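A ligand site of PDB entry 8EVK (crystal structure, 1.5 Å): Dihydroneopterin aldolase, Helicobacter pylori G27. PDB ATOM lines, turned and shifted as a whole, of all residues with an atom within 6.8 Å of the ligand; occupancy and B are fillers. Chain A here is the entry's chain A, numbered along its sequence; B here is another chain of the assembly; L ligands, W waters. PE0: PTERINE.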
ATOM      1  N   GLY A   9       6.630  13.694  -4.178  1.00  0.00           N
ATOM      2  CA  GLY A   9       6.443  14.672  -5.234  1.00  0.00           C
ATOM      3  C   GLY A   9       4.970  14.894  -5.539  1.00  0.00           C
ATOM      4  O   GLY A   9       4.138  14.000  -5.413  1.00  0.00           O
ATOM      5  N   VAL A  10       4.665  16.131  -5.918  1.00  0.00           N
ATOM      6  CA  VAL A  10       3.398  16.478  -6.548  1.00  0.00           C
ATOM      7  C   VAL A  10       3.720  16.971  -7.956  1.00  0.00           C
ATOM      8  O   VAL A  10       4.689  17.731  -8.158  1.00  0.00           O
ATOM      9  CB  VAL A  10       2.626  17.531  -5.735  1.00  0.00           C
ATOM     10  CG1 VAL A  10       1.382  17.950  -6.472  1.00  0.00           C
ATOM     11  CG2 VAL A  10       2.269  16.963  -4.370  1.00  0.00           C
ATOM     12  N   TYR A  42       9.272  17.165  -1.648  1.00  0.00           N
ATOM     13  CA  TYR A  42       9.442  17.457  -0.222  1.00  0.00           C
ATOM     14  C   TYR A  42       9.734  16.173   0.531  1.00  0.00           C
ATOM     15  O   TYR A  42       9.586  15.063   0.013  1.00  0.00           O
ATOM     16  CB  TYR A  42       8.216  18.148   0.353  1.00  0.00           C
ATOM     17  CG  TYR A  42       6.935  17.365   0.215  1.00  0.00           C
ATOM     18  CD1 TYR A  42       6.181  17.431  -0.957  1.00  0.00           C
ATOM     19  CD2 TYR A  42       6.488  16.544   1.246  1.00  0.00           C
ATOM     20  CE1 TYR A  42       5.008  16.712  -1.087  1.00  0.00           C
ATOM     21  CE2 TYR A  42       5.309  15.823   1.123  1.00  0.00           C
ATOM     22  CZ  TYR A  42       4.574  15.903  -0.041  1.00  0.00           C
ATOM     23  OH  TYR A  42       3.408  15.185  -0.164  1.00  0.00           O
ATOM     24  N   TYR A  50      -1.284  18.459   2.488  1.00  0.00           N
ATOM     25  CA  TYR A  50      -0.869  18.073   1.147  1.00  0.00           C
ATOM     26  C   TYR A  50      -0.692  19.330   0.318  1.00  0.00           C
ATOM     27  O   TYR A  50      -1.292  20.373   0.604  1.00  0.00           O
ATOM     28  CB  TYR A  50      -1.854  17.100   0.487  1.00  0.00           C
ATOM     29  CG  TYR A  50      -3.280  17.582   0.398  1.00  0.00           C
ATOM     30  CD1 TYR A  50      -4.123  17.529   1.510  1.00  0.00           C
ATOM     31  CD2 TYR A  50      -3.797  18.057  -0.794  1.00  0.00           C
ATOM     32  CE1 TYR A  50      -5.434  17.962   1.436  1.00  0.00           C
ATOM     33  CE2 TYR A  50      -5.123  18.489  -0.881  1.00  0.00           C
ATOM     34  CZ  TYR A  50      -5.929  18.434   0.236  1.00  0.00           C
ATOM     35  OH  TYR A  50      -7.245  18.856   0.154  1.00  0.00           O
ATOM     36  N   LEU A  51       0.181  19.239  -0.679  1.00  0.00           N
ATOM     37  CA  LEU A  51       0.350  20.319  -1.659  1.00  0.00           C
ATOM     38  C   LEU A  51      -0.740  20.134  -2.705  1.00  0.00           C
ATOM     39  O   LEU A  51      -0.645  19.265  -3.573  1.00  0.00           O
ATOM     40  CB  LEU A  51       1.746  20.293  -2.268  1.00  0.00           C
ATOM     41  CG  LEU A  51       2.972  20.127  -1.375  1.00  0.00           C
ATOM     42  CD1 LEU A  51       4.221  20.476  -2.162  1.00  0.00           C
ATOM     43  CD2 LEU A  51       2.908  20.981  -0.126  1.00  0.00           C
ATOM     44  N   ASP A  52      -1.790  20.934  -2.599  1.00  0.00           N
ATOM     45  CA  ASP A  52      -2.996  20.726  -3.383  1.00  0.00           C
ATOM     46  C   ASP A  52      -2.738  21.047  -4.852  1.00  0.00           C
ATOM     47  O   ASP A  52      -2.531  22.214  -5.216  1.00  0.00           O
ATOM     48  CB  ASP A  52      -4.085  21.635  -2.804  1.00  0.00           C
ATOM     49  CG  ASP A  52      -5.413  21.491  -3.507  1.00  0.00           C
ATOM     50  OD1 ASP A  52      -5.537  20.707  -4.457  1.00  0.00           O
ATOM     51  OD2 ASP A  52      -6.364  22.196  -3.084  1.00  0.00           O
ATOM     52  N   TYR A  53      -2.759  20.025  -5.710  1.00  0.00           N
ATOM     53  CA  TYR A  53      -2.530  20.261  -7.138  1.00  0.00           C
ATOM     54  C   TYR A  53      -3.564  21.197  -7.744  1.00  0.00           C
ATOM     55  O   TYR A  53      -3.284  21.832  -8.766  1.00  0.00           O
ATOM     56  CB  TYR A  53      -2.395  18.954  -7.928  1.00  0.00           C
ATOM     57  CG  TYR A  53      -3.569  17.997  -7.838  1.00  0.00           C
ATOM     58  CD1 TYR A  53      -4.797  18.312  -8.404  1.00  0.00           C
ATOM     59  CD2 TYR A  53      -3.438  16.765  -7.197  1.00  0.00           C
ATOM     60  CE1 TYR A  53      -5.878  17.450  -8.323  1.00  0.00           C
ATOM     61  CE2 TYR A  53      -4.514  15.883  -7.118  1.00  0.00           C
ATOM     62  CZ  TYR A  53      -5.731  16.243  -7.686  1.00  0.00           C
ATOM     63  OH  TYR A  53      -6.814  15.393  -7.618  1.00  0.00           O
ATOM     64  N   ILE A  54      -4.741  21.314  -7.131  1.00  0.00           N
ATOM     65  CA  ILE A  54      -5.773  22.225  -7.633  1.00  0.00           C
ATOM     66  C   ILE A  54      -5.311  23.679  -7.492  1.00  0.00           C
ATOM     67  O   ILE A  54      -5.323  24.448  -8.464  1.00  0.00           O
ATOM     68  CB  ILE A  54      -7.115  21.980  -6.920  1.00  0.00           C
ATOM     69  CG1 ILE A  54      -7.737  20.662  -7.406  1.00  0.00           C
ATOM     70  CG2 ILE A  54      -8.069  23.152  -7.166  1.00  0.00           C
ATOM     71  CD1 ILE A  54      -7.857  20.548  -8.905  1.00  0.00           C
ATOM     72  N   LYS A  55      -4.932  24.070  -6.273  1.00  0.00           N
ATOM     73  CA  LYS A  55      -4.423  25.424  -6.083  1.00  0.00           C
ATOM     74  C   LYS A  55      -3.207  25.655  -6.968  1.00  0.00           C
ATOM     75  O   LYS A  55      -3.093  26.707  -7.620  1.00  0.00           O
ATOM     76  CB  LYS A  55      -4.094  25.663  -4.617  1.00  0.00           C
ATOM     77  CG  LYS A  55      -5.207  25.250  -3.662  1.00  0.00           C
ATOM     78  CD  LYS A  55      -5.294  26.166  -2.453  1.00  0.00           C
ATOM     79  CE  LYS A  55      -6.278  25.624  -1.415  1.00  0.00           C
ATOM     80  NZ  LYS A  55      -5.873  24.289  -0.912  1.00  0.00           N
ATOM     81  N   ILE A  56      -2.317  24.671  -7.059  1.00  0.00           N
ATOM     82  CA  ILE A  56      -1.042  24.866  -7.738  1.00  0.00           C
ATOM     83  C   ILE A  56      -1.282  25.206  -9.201  1.00  0.00           C
ATOM     84  O   ILE A  56      -0.712  26.161  -9.744  1.00  0.00           O
ATOM     85  CB  ILE A  56      -0.165  23.605  -7.578  1.00  0.00           C
ATOM     86  CG1 ILE A  56       0.379  23.516  -6.146  1.00  0.00           C
ATOM     87  CG2 ILE A  56       0.983  23.648  -8.561  1.00  0.00           C
ATOM     88  CD1 ILE A  56       0.925  22.143  -5.807  1.00  0.00           C
ATOM     89  N   LEU B  21     -11.036   6.927  -5.590  1.00  0.00           N
ATOM     90  CA  LEU B  21      -9.879   7.617  -5.070  1.00  0.00           C
ATOM     91  C   LEU B  21     -10.237   9.085  -4.973  1.00  0.00           C
ATOM     92  O   LEU B  21     -10.891   9.633  -5.875  1.00  0.00           O
ATOM     93  CB  LEU B  21      -8.708   7.469  -6.058  1.00  0.00           C
ATOM     94  CG  LEU B  21      -7.437   8.253  -5.790  1.00  0.00           C
ATOM     95  CD1 LEU B  21      -6.774   7.787  -4.507  1.00  0.00           C
ATOM     96  CD2 LEU B  21      -6.458   8.030  -6.932  1.00  0.00           C
ATOM     97  N   GLY B  22      -9.849   9.726  -3.895  1.00  0.00           N
ATOM     98  CA  GLY B  22     -10.029  11.157  -3.765  1.00  0.00           C
ATOM     99  C   GLY B  22     -10.459  11.609  -2.400  1.00  0.00           C
ATOM    100  O   GLY B  22     -11.089  10.879  -1.639  1.00  0.00           O
ATOM    101  N   ILE B  23     -10.116  12.855  -2.078  1.00  0.00           N
ATOM    102  CA  ILE B  23     -10.525  13.481  -0.814  1.00  0.00           C
ATOM    103  C   ILE B  23     -11.708  14.434  -0.980  1.00  0.00           C
ATOM    104  O   ILE B  23     -12.346  14.787   0.014  1.00  0.00           O
ATOM    105  CB  ILE B  23      -9.320  14.171  -0.139  1.00  0.00           C
ATOM    106  CG1 ILE B  23      -9.604  14.454   1.337  1.00  0.00           C
ATOM    107  CG2 ILE B  23      -8.932  15.437  -0.903  1.00  0.00           C
ATOM    108  CD1 ILE B  23      -8.580  15.353   1.992  1.00  0.00           C
ATOM    109  N   LEU B  24     -12.020  14.838  -2.208  1.00  0.00           N
ATOM    110  CA  LEU B  24     -13.220  15.635  -2.471  1.00  0.00           C
ATOM    111  C   LEU B  24     -14.429  14.719  -2.660  1.00  0.00           C
ATOM    112  O   LEU B  24     -14.362  13.716  -3.364  1.00  0.00           O
ATOM    113  CB  LEU B  24     -13.020  16.482  -3.726  1.00  0.00           C
ATOM    114  CG  LEU B  24     -11.876  17.499  -3.627  1.00  0.00           C
ATOM    115  CD1 LEU B  24     -11.659  18.205  -4.958  1.00  0.00           C
ATOM    116  CD2 LEU B  24     -12.146  18.501  -2.524  1.00  0.00           C
ATOM    117  N   GLU B  27     -15.609  13.193  -5.993  1.00  0.00           N
ATOM    118  CA  GLU B  27     -14.766  12.224  -6.700  1.00  0.00           C
ATOM    119  C   GLU B  27     -15.049  10.810  -6.255  1.00  0.00           C
ATOM    120  O   GLU B  27     -14.854   9.868  -7.031  1.00  0.00           O
ATOM    121  CB  GLU B  27     -13.309  12.537  -6.390  1.00  0.00           C
ATOM    122  CG  GLU B  27     -12.743  13.582  -7.279  1.00  0.00           C
ATOM    123  CD  GLU B  27     -11.252  13.731  -7.078  1.00  0.00           C
ATOM    124  OE1 GLU B  27     -10.520  12.791  -7.431  1.00  0.00           O
ATOM    125  OE2 GLU B  27     -10.837  14.790  -6.562  1.00  0.00           O
ATOM    126  N   LEU B  70      -8.120   8.015   0.139  1.00  0.00           N
ATOM    127  CA  LEU B  70      -8.491   9.422   0.064  1.00  0.00           C
ATOM    128  C   LEU B  70      -7.473  10.192  -0.782  1.00  0.00           C
ATOM    129  O   LEU B  70      -7.669  10.351  -1.992  1.00  0.00           O
ATOM    130  CB  LEU B  70      -8.618   9.987   1.487  1.00  0.00           C
ATOM    131  CG  LEU B  70      -9.767   9.368   2.297  1.00  0.00           C
ATOM    132  CD1 LEU B  70      -9.605   9.639   3.779  1.00  0.00           C
ATOM    133  CD2 LEU B  70     -11.100   9.895   1.822  1.00  0.00           C
ATOM    134  N   LEU B  71      -6.396  10.674  -0.169  1.00  0.00           N
ATOM    135  CA  LEU B  71      -5.355  11.357  -0.942  1.00  0.00           C
ATOM    136  C   LEU B  71      -4.543  10.353  -1.745  1.00  0.00           C
ATOM    137  O   LEU B  71      -4.392   9.184  -1.368  1.00  0.00           O
ATOM    138  CB  LEU B  71      -4.403  12.084   0.003  1.00  0.00           C
ATOM    139  CG  LEU B  71      -4.989  13.293   0.746  1.00  0.00           C
ATOM    140  CD1 LEU B  71      -4.093  13.699   1.890  1.00  0.00           C
ATOM    141  CD2 LEU B  71      -5.233  14.461  -0.210  1.00  0.00           C
ATOM    142  N   ILE B  72      -4.022  10.813  -2.891  1.00  0.00           N
ATOM    143  CA  ILE B  72      -3.046   9.991  -3.610  1.00  0.00           C
ATOM    144  C   ILE B  72      -1.904   9.633  -2.665  1.00  0.00           C
ATOM    145  O   ILE B  72      -1.412   8.502  -2.663  1.00  0.00           O
ATOM    146  CB  ILE B  72      -2.502  10.738  -4.842  1.00  0.00           C
ATOM    147  CG1 ILE B  72      -3.641  11.116  -5.777  1.00  0.00           C
ATOM    148  CG2 ILE B  72      -1.460   9.881  -5.570  1.00  0.00           C
ATOM    149  CD1 ILE B  72      -3.197  11.987  -6.945  1.00  0.00           C
ATOM    150  N   GLU B  73      -1.500  10.602  -1.832  1.00  0.00           N
ATOM    151  CA  GLU B  73      -0.414  10.386  -0.887  1.00  0.00           C
ATOM    152  C   GLU B  73      -0.744   9.279   0.093  1.00  0.00           C
ATOM    153  O   GLU B  73       0.156   8.581   0.553  1.00  0.00           O
ATOM    154  CB  GLU B  73      -0.119  11.708  -0.165  1.00  0.00           C
ATOM    155  CG  GLU B  73       0.583  12.800  -1.014  1.00  0.00           C
ATOM    156  CD  GLU B  73      -0.351  13.569  -1.963  1.00  0.00           C
ATOM    157  OE1 GLU B  73      -1.557  13.244  -2.069  1.00  0.00           O
ATOM    158  OE2 GLU B  73       0.127  14.529  -2.614  1.00  0.00           O
ATOM    159  N   ASP B  74      -2.030   9.081   0.416  1.00  0.00           N
ATOM    160  CA  ASP B  74      -2.400   7.971   1.276  1.00  0.00           C
ATOM    161  C   ASP B  74      -2.167   6.632   0.576  1.00  0.00           C
ATOM    162  O   ASP B  74      -1.648   5.692   1.179  1.00  0.00           O
ATOM    163  CB  ASP B  74      -3.883   8.090   1.673  1.00  0.00           C
ATOM    164  CG  ASP B  74      -4.164   9.287   2.559  1.00  0.00           C
ATOM    165  OD1 ASP B  74      -3.259   9.696   3.338  1.00  0.00           O
ATOM    166  OD2 ASP B  74      -5.294   9.845   2.482  1.00  0.00           O
ATOM    167  N   LYS B  99      -4.079  10.934 -11.880  1.00  0.00           N
ATOM    168  CA  LYS B  99      -5.513  11.019 -12.183  1.00  0.00           C
ATOM    169  C   LYS B  99      -5.659  11.551 -13.606  1.00  0.00           C
ATOM    170  O   LYS B  99      -5.306  12.697 -13.875  1.00  0.00           O
ATOM    171  CB  LYS B  99      -6.219  11.939 -11.205  1.00  0.00           C
ATOM    172  CG  LYS B  99      -6.395  11.347  -9.812  1.00  0.00           C
ATOM    173  CD  LYS B  99      -7.108  12.343  -8.939  1.00  0.00           C
ATOM    174  CE  LYS B  99      -7.254  11.846  -7.514  1.00  0.00           C
ATOM    175  NZ  LYS B  99      -7.766  12.916  -6.615  1.00  0.00           N
ATOM    176  N   ILE B 102      -9.279  14.092 -13.960  1.00  0.00           N
ATOM    177  CA  ILE B 102      -9.739  15.020 -12.926  1.00  0.00           C
ATOM    178  C   ILE B 102      -9.674  16.468 -13.388  1.00  0.00           C
ATOM    179  O   ILE B 102     -10.378  17.315 -12.834  1.00  0.00           O
ATOM    180  CB  ILE B 102      -8.984  14.788 -11.605  1.00  0.00           C
ATOM    181  CG1 ILE B 102      -9.755  15.396 -10.434  1.00  0.00           C
ATOM    182  CG2 ILE B 102      -7.599  15.379 -11.690  1.00  0.00           C
ATOM    183  CD1 ILE B 102     -11.121  14.805 -10.249  1.00  0.00           C
ATOM    184  N   GLY B 109      -0.645  14.318 -10.584  1.00  0.00           N
ATOM    185  CA  GLY B 109      -0.324  13.090  -9.883  1.00  0.00           C
ATOM    186  C   GLY B 109       0.579  13.379  -8.705  1.00  0.00           C
ATOM    187  O   GLY B 109       0.945  14.522  -8.425  1.00  0.00           O
ATOM    188  N   ALA B 110       0.906  12.315  -7.983  1.00  0.00           N
ATOM    189  CA  ALA B 110       1.822  12.388  -6.869  1.00  0.00           C
ATOM    190  C   ALA B 110       2.695  11.145  -6.913  1.00  0.00           C
ATOM    191  O   ALA B 110       2.275  10.106  -7.426  1.00  0.00           O
ATOM    192  CB  ALA B 110       1.104  12.516  -5.513  1.00  0.00           C
HETATM  193  C1  PE0 L   1      -5.413  15.732  -4.101  1.00  0.00           C
HETATM  194  C4  PE0 L   1      -4.562  14.643  -3.738  1.00  0.00           C
HETATM  195  O4  PE0 L   1      -4.955  13.479  -3.690  1.00  0.00           O
HETATM  196  N2  PE0 L   1      -3.277  15.031  -3.650  1.00  0.00           N
HETATM  197  C3  PE0 L   1      -2.803  16.299  -3.783  1.00  0.00           C
HETATM  198  N6  PE0 L   1      -1.489  16.486  -3.616  1.00  0.00           N
HETATM  199  N1  PE0 L   1      -3.561  17.285  -4.072  1.00  0.00           N
HETATM  200  C2  PE0 L   1      -4.848  17.012  -4.245  1.00  0.00           C
HETATM  201  N3  PE0 L   1      -5.664  17.971  -4.513  1.00  0.00           N
HETATM  202  C6  PE0 L   1      -6.884  17.750  -4.719  1.00  0.00           C
HETATM  203  C5  PE0 L   1      -7.399  16.552  -4.639  1.00  0.00           C
HETATM  204  N4  PE0 L   1      -6.680  15.585  -4.323  1.00  0.00           N
HETATM  205  O   HOH W   1      -8.530  19.787  -2.487  1.00  0.00           O
HETATM  206  O   HOH W   2      -6.993  11.825  -4.333  1.00  0.00           O
HETATM  207  O   HOH W   3      -9.402  14.433  -4.280  1.00  0.00           O
HETATM  208  O   HOH W   4      -9.211  16.661  -7.093  1.00  0.00           O
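OE2 of Glu 73 of chain B lies within hydrogen-bond range of N6 of the ligand, 2.7 Å away. The backbone carbonyl oxygen (O) of Leu 51 sits at hydrogen-bond distance from a nitrogen (N6) of the ligand, 2.9 Å away. N of Tyr 53 lies close to N1 of the ligand (3.3 Å). OH of Tyr 53 sits close to N4 of the ligand. A nitrogen (N3) of the ligand sits at hydrogen-bond distance from the side-chain carboxylate (OD1) of Asp 52 (2.7 Å). N of Ile 72 of chain B lies within hydrogen-bond range of O4 of the ligand.
OD2 of Asp 52 is in salt-bridge range of NZ of Lys 55, at 3.1 Å. NZ of Lys 99 of chain B lies within salt-bridge range of OE1 of Glu 27 of chain B, at 2.9 Å. The side-chain hydroxyl (OH) of Tyr 53 lies within hydrogen-bond range of the side-chain amino group (NZ) of Lys 99 of chain B (2.8 Å). The side-chain carboxylate (OD1) of Asp 52 sits at hydrogen-bond distance from the backbone NH (N) of Ile 54, at 2.9 Å. The backbone NH (N) of Leu 71 of chain B sits at hydrogen-bond distance from the side-chain carboxylate (OD2) of Asp 74 of chain B (3.0 Å).
CG2 of Val 10 touches N6 of the ligand, at 3.9 Å. Tyr 50 touches the ligand (CD2 to N1, 3.4 Å). Leu 71 of chain B touches the ligand (CA to O4, 3.5 Å). Lys 99 of chain B touches the ligand (NZ to N4, 3.7 Å). Hydrophobic or aromatic side chains that line the ligand: Val 10, Tyr 50, Tyr 53, Leu 71 of chain B and Ile 72 of chain B. Within 4 Å of the ligand: Val 10, Tyr 50, Leu 51, Asp 52, Tyr 53, Leu 71 of chain B, Ile 72 of chain B, Glu 73 of chain B and Lys 99 of chain B. The nearest printed residue that does not touch the ligand is Ile 54 (4.1 Å).
Water W2 lies within hydrogen-bond range of NZ of Lys 99 of chain B (2.6 Å), O4 of the ligand (2.7 Å), O of Leu 70 of chain B (2.8 Å) and N of Ile 72 of chain B (3.5 Å). Water W4 lies within hydrogen-bond range of OE2 of Glu 27 of chain B and OH of Tyr 53. Water W1 lies within hydrogen-bond range of the side-chain hydroxyl of Tyr 50 (3.1 Å) and the side-chain carboxylate of Asp 52 (3.3 Å).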
